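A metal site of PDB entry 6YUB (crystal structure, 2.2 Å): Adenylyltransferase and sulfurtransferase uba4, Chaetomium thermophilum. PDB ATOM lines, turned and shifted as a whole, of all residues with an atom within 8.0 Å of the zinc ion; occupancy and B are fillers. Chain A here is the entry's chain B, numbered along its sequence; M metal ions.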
ATOM      1  N   SER A 142     -33.255  10.582 -19.447  1.00  0.00           N
ATOM      2  CA  SER A 142     -32.786  10.744 -20.816  1.00  0.00           C
ATOM      3  C   SER A 142     -31.424  10.081 -21.018  1.00  0.00           C
ATOM      4  O   SER A 142     -31.241   9.278 -21.939  1.00  0.00           O
ATOM      5  CB  SER A 142     -32.730  12.223 -21.170  1.00  0.00           C
ATOM      6  OG  SER A 142     -32.607  12.411 -22.580  1.00  0.00           O
ATOM      7  N   ASP A 143     -30.465  10.410 -20.163  1.00  0.00           N
ATOM      8  CA  ASP A 143     -29.136   9.822 -20.267  1.00  0.00           C
ATOM      9  C   ASP A 143     -29.206   8.301 -20.306  1.00  0.00           C
ATOM     10  O   ASP A 143     -28.646   7.661 -21.206  1.00  0.00           O
ATOM     11  CB  ASP A 143     -28.258  10.299 -19.108  1.00  0.00           C
ATOM     12  CG  ASP A 143     -27.919  11.787 -19.220  1.00  0.00           C
ATOM     13  OD1 ASP A 143     -28.217  12.388 -20.269  1.00  0.00           O
ATOM     14  OD2 ASP A 143     -27.350  12.341 -18.259  1.00  0.00           O
ATOM     15  N   VAL A 146     -30.651   6.903 -23.479  1.00  0.00           N
ATOM     16  CA  VAL A 146     -29.677   6.936 -24.563  1.00  0.00           C
ATOM     17  C   VAL A 146     -28.700   5.787 -24.444  1.00  0.00           C
ATOM     18  O   VAL A 146     -28.384   5.108 -25.437  1.00  0.00           O
ATOM     19  CB  VAL A 146     -28.945   8.300 -24.566  1.00  0.00           C
ATOM     20  CG1 VAL A 146     -27.657   8.209 -25.356  1.00  0.00           C
ATOM     21  CG2 VAL A 146     -29.861   9.377 -25.122  1.00  0.00           C
ATOM     22  N   LEU A 167     -38.532  11.213 -27.421  1.00  0.00           N
ATOM     23  CA  LEU A 167     -37.091  11.321 -27.583  1.00  0.00           C
ATOM     24  C   LEU A 167     -36.492   9.957 -27.895  1.00  0.00           C
ATOM     25  O   LEU A 167     -37.020   8.918 -27.487  1.00  0.00           O
ATOM     26  CB  LEU A 167     -36.436  11.895 -26.302  1.00  0.00           C
ATOM     27  CG  LEU A 167     -36.933  13.267 -25.860  1.00  0.00           C
ATOM     28  CD1 LEU A 167     -36.582  13.528 -24.402  1.00  0.00           C
ATOM     29  CD2 LEU A 167     -36.351  14.363 -26.754  1.00  0.00           C
ATOM     30  N   ALA A 182     -32.720  10.610 -33.803  1.00  0.00           N
ATOM     31  CA  ALA A 182     -33.598  11.385 -32.942  1.00  0.00           C
ATOM     32  C   ALA A 182     -32.789  12.017 -31.815  1.00  0.00           C
ATOM     33  O   ALA A 182     -31.750  11.494 -31.400  1.00  0.00           O
ATOM     34  CB  ALA A 182     -34.690  10.497 -32.361  1.00  0.00           C
ATOM     35  N   PRO A 183     -33.249  13.150 -31.287  1.00  0.00           N
ATOM     36  CA  PRO A 183     -32.518  13.816 -30.202  1.00  0.00           C
ATOM     37  C   PRO A 183     -32.771  13.167 -28.859  1.00  0.00           C
ATOM     38  O   PRO A 183     -33.712  12.388 -28.667  1.00  0.00           O
ATOM     39  CB  PRO A 183     -33.080  15.239 -30.233  1.00  0.00           C
ATOM     40  CG  PRO A 183     -34.494  15.059 -30.685  1.00  0.00           C
ATOM     41  CD  PRO A 183     -34.469  13.893 -31.670  1.00  0.00           C
ATOM     42  N   CYS A 184     -31.881  13.484 -27.911  1.00  0.00           N
ATOM     43  CA  CYS A 184     -32.117  13.194 -26.511  1.00  0.00           C
ATOM     44  C   CYS A 184     -32.577  14.483 -25.817  1.00  0.00           C
ATOM     45  O   CYS A 184     -32.673  15.555 -26.435  1.00  0.00           O
ATOM     46  CB  CYS A 184     -30.862  12.620 -25.861  1.00  0.00           C
ATOM     47  SG  CYS A 184     -29.818  13.844 -25.078  1.00  0.00           S
ATOM     48  N   TYR A 185     -32.849  14.390 -24.512  1.00  0.00           N
ATOM     49  CA  TYR A 185     -33.356  15.560 -23.799  1.00  0.00           C
ATOM     50  C   TYR A 185     -32.313  16.676 -23.729  1.00  0.00           C
ATOM     51  O   TYR A 185     -32.684  17.858 -23.713  1.00  0.00           O
ATOM     52  CB  TYR A 185     -33.804  15.165 -22.386  1.00  0.00           C
ATOM     53  CG  TYR A 185     -34.610  16.223 -21.668  1.00  0.00           C
ATOM     54  CD1 TYR A 185     -35.970  16.400 -21.939  1.00  0.00           C
ATOM     55  CD2 TYR A 185     -34.026  17.047 -20.726  1.00  0.00           C
ATOM     56  CE1 TYR A 185     -36.708  17.364 -21.285  1.00  0.00           C
ATOM     57  CE2 TYR A 185     -34.761  18.025 -20.073  1.00  0.00           C
ATOM     58  CZ  TYR A 185     -36.103  18.177 -20.352  1.00  0.00           C
ATOM     59  OH  TYR A 185     -36.828  19.146 -19.698  1.00  0.00           O
ATOM     60  N   ARG A 186     -31.021  16.330 -23.686  1.00  0.00           N
ATOM     61  CA  ARG A 186     -29.994  17.361 -23.688  1.00  0.00           C
ATOM     62  C   ARG A 186     -29.893  18.036 -25.051  1.00  0.00           C
ATOM     63  O   ARG A 186     -29.672  19.244 -25.134  1.00  0.00           O
ATOM     64  CB  ARG A 186     -28.637  16.758 -23.302  1.00  0.00           C
ATOM     65  CG  ARG A 186     -28.505  16.419 -21.829  1.00  0.00           C
ATOM     66  CD  ARG A 186     -27.173  15.737 -21.550  1.00  0.00           C
ATOM     67  NE  ARG A 186     -27.121  15.163 -20.210  1.00  0.00           N
ATOM     68  CZ  ARG A 186     -26.725  15.818 -19.123  1.00  0.00           C
ATOM     69  NH1 ARG A 186     -26.337  17.082 -19.206  1.00  0.00           N
ATOM     70  NH2 ARG A 186     -26.715  15.201 -17.957  1.00  0.00           N
ATOM     71  N   CYS A 187     -30.067  17.269 -26.137  1.00  0.00           N
ATOM     72  CA  CYS A 187     -30.068  17.848 -27.474  1.00  0.00           C
ATOM     73  C   CYS A 187     -31.056  19.001 -27.565  1.00  0.00           C
ATOM     74  O   CYS A 187     -30.836  19.952 -28.324  1.00  0.00           O
ATOM     75  CB  CYS A 187     -30.416  16.784 -28.518  1.00  0.00           C
ATOM     76  SG  CYS A 187     -29.177  15.521 -28.801  1.00  0.00           S
ATOM     77  N   CYS A 188     -32.160  18.927 -26.815  1.00  0.00           N
ATOM     78  CA  CYS A 188     -33.220  19.927 -26.909  1.00  0.00           C
ATOM     79  C   CYS A 188     -33.064  21.047 -25.895  1.00  0.00           C
ATOM     80  O   CYS A 188     -33.372  22.211 -26.204  1.00  0.00           O
ATOM     81  CB  CYS A 188     -34.580  19.259 -26.704  1.00  0.00           C
ATOM     82  SG  CYS A 188     -34.936  17.878 -27.806  1.00  0.00           S
ATOM     83  N   PHE A 189     -32.588  20.736 -24.680  1.00  0.00           N
ATOM     84  CA  PHE A 189     -32.592  21.701 -23.584  1.00  0.00           C
ATOM     85  C   PHE A 189     -31.258  21.705 -22.867  1.00  0.00           C
ATOM     86  O   PHE A 189     -30.731  20.638 -22.534  1.00  0.00           O
ATOM     87  CB  PHE A 189     -33.710  21.374 -22.584  1.00  0.00           C
ATOM     88  CG  PHE A 189     -35.041  21.121 -23.223  1.00  0.00           C
ATOM     89  CD1 PHE A 189     -35.697  22.125 -23.911  1.00  0.00           C
ATOM     90  CD2 PHE A 189     -35.639  19.873 -23.139  1.00  0.00           C
ATOM     91  CE1 PHE A 189     -36.924  21.890 -24.513  1.00  0.00           C
ATOM     92  CE2 PHE A 189     -36.868  19.639 -23.725  1.00  0.00           C
ATOM     93  CZ  PHE A 189     -37.510  20.648 -24.412  1.00  0.00           C
ATOM     94  N   GLY A 274     -32.690  17.310 -34.786  1.00  0.00           N
ATOM     95  CA  GLY A 274     -32.234  15.957 -34.542  1.00  0.00           C
ATOM     96  C   GLY A 274     -31.105  15.917 -33.532  1.00  0.00           C
ATOM     97  O   GLY A 274     -30.780  16.899 -32.863  1.00  0.00           O
ATOM     98  N   ARG A 275     -30.500  14.734 -33.419  1.00  0.00           N
ATOM     99  CA  ARG A 275     -29.373  14.552 -32.523  1.00  0.00           C
ATOM    100  C   ARG A 275     -28.275  15.564 -32.843  1.00  0.00           C
ATOM    101  O   ARG A 275     -27.893  15.744 -34.000  1.00  0.00           O
ATOM    102  CB  ARG A 275     -28.822  13.125 -32.650  1.00  0.00           C
ATOM    103  CG  ARG A 275     -27.425  12.939 -32.086  1.00  0.00           C
ATOM    104  CD  ARG A 275     -27.024  11.471 -32.107  1.00  0.00           C
ATOM    105  NE  ARG A 275     -27.799  10.685 -31.152  1.00  0.00           N
ATOM    106  CZ  ARG A 275     -27.730   9.362 -31.040  1.00  0.00           C
ATOM    107  NH1 ARG A 275     -26.917   8.667 -31.812  1.00  0.00           N
ATOM    108  NH2 ARG A 275     -28.476   8.734 -30.138  1.00  0.00           N
ATOM    109  N   LYS A 276     -27.784  16.236 -31.802  1.00  0.00           N
ATOM    110  CA  LYS A 276     -26.673  17.166 -31.965  1.00  0.00           C
ATOM    111  C   LYS A 276     -25.353  16.418 -31.963  1.00  0.00           C
ATOM    112  O   LYS A 276     -25.140  15.513 -31.160  1.00  0.00           O
ATOM    113  CB  LYS A 276     -26.698  18.228 -30.859  1.00  0.00           C
ATOM    114  CG  LYS A 276     -27.692  19.361 -31.100  1.00  0.00           C
ATOM    115  CD  LYS A 276     -27.540  20.468 -30.069  1.00  0.00           C
ATOM    116  CE  LYS A 276     -26.214  21.216 -30.206  1.00  0.00           C
ATOM    117  NZ  LYS A 276     -25.597  21.496 -28.883  1.00  0.00           N
ATOM    118  N   LYS A 277     -24.456  16.817 -32.863  1.00  0.00           N
ATOM    119  CA  LYS A 277     -23.185  16.123 -32.995  1.00  0.00           C
ATOM    120  C   LYS A 277     -22.319  16.290 -31.751  1.00  0.00           C
ATOM    121  O   LYS A 277     -21.482  15.432 -31.451  1.00  0.00           O
ATOM    122  CB  LYS A 277     -22.434  16.629 -34.232  1.00  0.00           C
ATOM    123  CG  LYS A 277     -21.262  15.754 -34.635  1.00  0.00           C
ATOM    124  CD  LYS A 277     -20.935  15.873 -36.124  1.00  0.00           C
ATOM    125  CE  LYS A 277     -20.347  17.235 -36.469  1.00  0.00           C
ATOM    126  NZ  LYS A 277     -19.646  17.207 -37.786  1.00  0.00           N
ATOM    127  N   ASP A 278     -22.506  17.381 -31.008  1.00  0.00           N
ATOM    128  CA  ASP A 278     -21.690  17.677 -29.838  1.00  0.00           C
ATOM    129  C   ASP A 278     -22.468  17.545 -28.536  1.00  0.00           C
ATOM    130  O   ASP A 278     -22.134  18.179 -27.535  1.00  0.00           O
ATOM    131  CB  ASP A 278     -21.103  19.084 -29.943  1.00  0.00           C
ATOM    132  CG  ASP A 278     -22.166  20.163 -29.850  1.00  0.00           C
ATOM    133  OD1 ASP A 278     -23.338  19.879 -30.184  1.00  0.00           O
ATOM    134  OD2 ASP A 278     -21.828  21.298 -29.432  1.00  0.00           O
ATOM    135  N   CYS A 279     -23.525  16.722 -28.525  1.00  0.00           N
ATOM    136  CA  CYS A 279     -24.327  16.569 -27.323  1.00  0.00           C
ATOM    137  C   CYS A 279     -23.528  15.850 -26.244  1.00  0.00           C
ATOM    138  O   CYS A 279     -22.901  14.814 -26.503  1.00  0.00           O
ATOM    139  CB  CYS A 279     -25.605  15.803 -27.616  1.00  0.00           C
ATOM    140  SG  CYS A 279     -26.469  15.292 -26.110  1.00  0.00           S
ATOM    141  N   PHE A 280     -23.570  16.381 -25.024  1.00  0.00           N
ATOM    142  CA  PHE A 280     -22.834  15.789 -23.911  1.00  0.00           C
ATOM    143  C   PHE A 280     -23.130  14.302 -23.773  1.00  0.00           C
ATOM    144  O   PHE A 280     -22.231  13.514 -23.425  1.00  0.00           O
ATOM    145  CB  PHE A 280     -23.188  16.523 -22.616  1.00  0.00           C
ATOM    146  CG  PHE A 280     -22.668  15.861 -21.372  1.00  0.00           C
ATOM    147  CD1 PHE A 280     -21.364  16.060 -20.958  1.00  0.00           C
ATOM    148  CD2 PHE A 280     -23.487  15.061 -20.600  1.00  0.00           C
ATOM    149  CE1 PHE A 280     -20.883  15.458 -19.814  1.00  0.00           C
ATOM    150  CE2 PHE A 280     -23.009  14.446 -19.455  1.00  0.00           C
ATOM    151  CZ  PHE A 280     -21.697  14.649 -19.064  1.00  0.00           C
ATOM    152  N   ALA A 281     -24.365  13.888 -24.041  1.00  0.00           N
ATOM    153  CA  ALA A 281     -24.813  12.528 -23.766  1.00  0.00           C
ATOM    154  C   ALA A 281     -24.800  11.621 -24.986  1.00  0.00           C
ATOM    155  O   ALA A 281     -24.243  10.516 -24.927  1.00  0.00           O
ATOM    156  CB  ALA A 281     -26.232  12.556 -23.157  1.00  0.00           C
ATOM    157  N   CYS A 282     -25.424  12.049 -26.086  1.00  0.00           N
ATOM    158  CA  CYS A 282     -25.565  11.207 -27.270  1.00  0.00           C
ATOM    159  C   CYS A 282     -24.669  11.633 -28.427  1.00  0.00           C
ATOM    160  O   CYS A 282     -24.674  10.973 -29.477  1.00  0.00           O
ATOM    161  CB  CYS A 282     -27.030  11.187 -27.730  1.00  0.00           C
ATOM    162  SG  CYS A 282     -27.747  12.794 -28.165  1.00  0.00           S
ATOM    163  N   GLY A 283     -23.892  12.700 -28.272  1.00  0.00           N
ATOM    164  CA  GLY A 283     -23.097  13.225 -29.356  1.00  0.00           C
ATOM    165  C   GLY A 283     -21.817  12.461 -29.587  1.00  0.00           C
ATOM    166  O   GLY A 283     -21.502  11.466 -28.933  1.00  0.00           O
HETATM  167 ZN    ZN M   1     -28.496  14.425 -26.876  1.00  0.00          ZN
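The side-chain sulfur (SG) of Cys 282 sits close to the guanidinium group (NE) of Arg 275. The backbone NH (N) of Arg 186 lies close to the side-chain sulfur (SG) of Cys 184 (3.1 Å). The backbone carbonyl oxygen (O) of Cys 184 lies within hydrogen-bond range of the side-chain sulfur (SG) of Cys 188, 3.5 Å away. SG of Cys 187 sits close to N of Lys 276, at 3.4 Å. SG of Cys 279 sits close to N of Ala 281 (3.3 Å).
Along chain A the residues within 4 Å of the zinc ion span positions 184 to 282.
The zinc ion is bound by SG of Cys 282 (2.2 Å), SG of Cys 184 (2.3 Å), SG of Cys 187 (2.3 Å) and SG of Cys 279 (2.3 Å).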
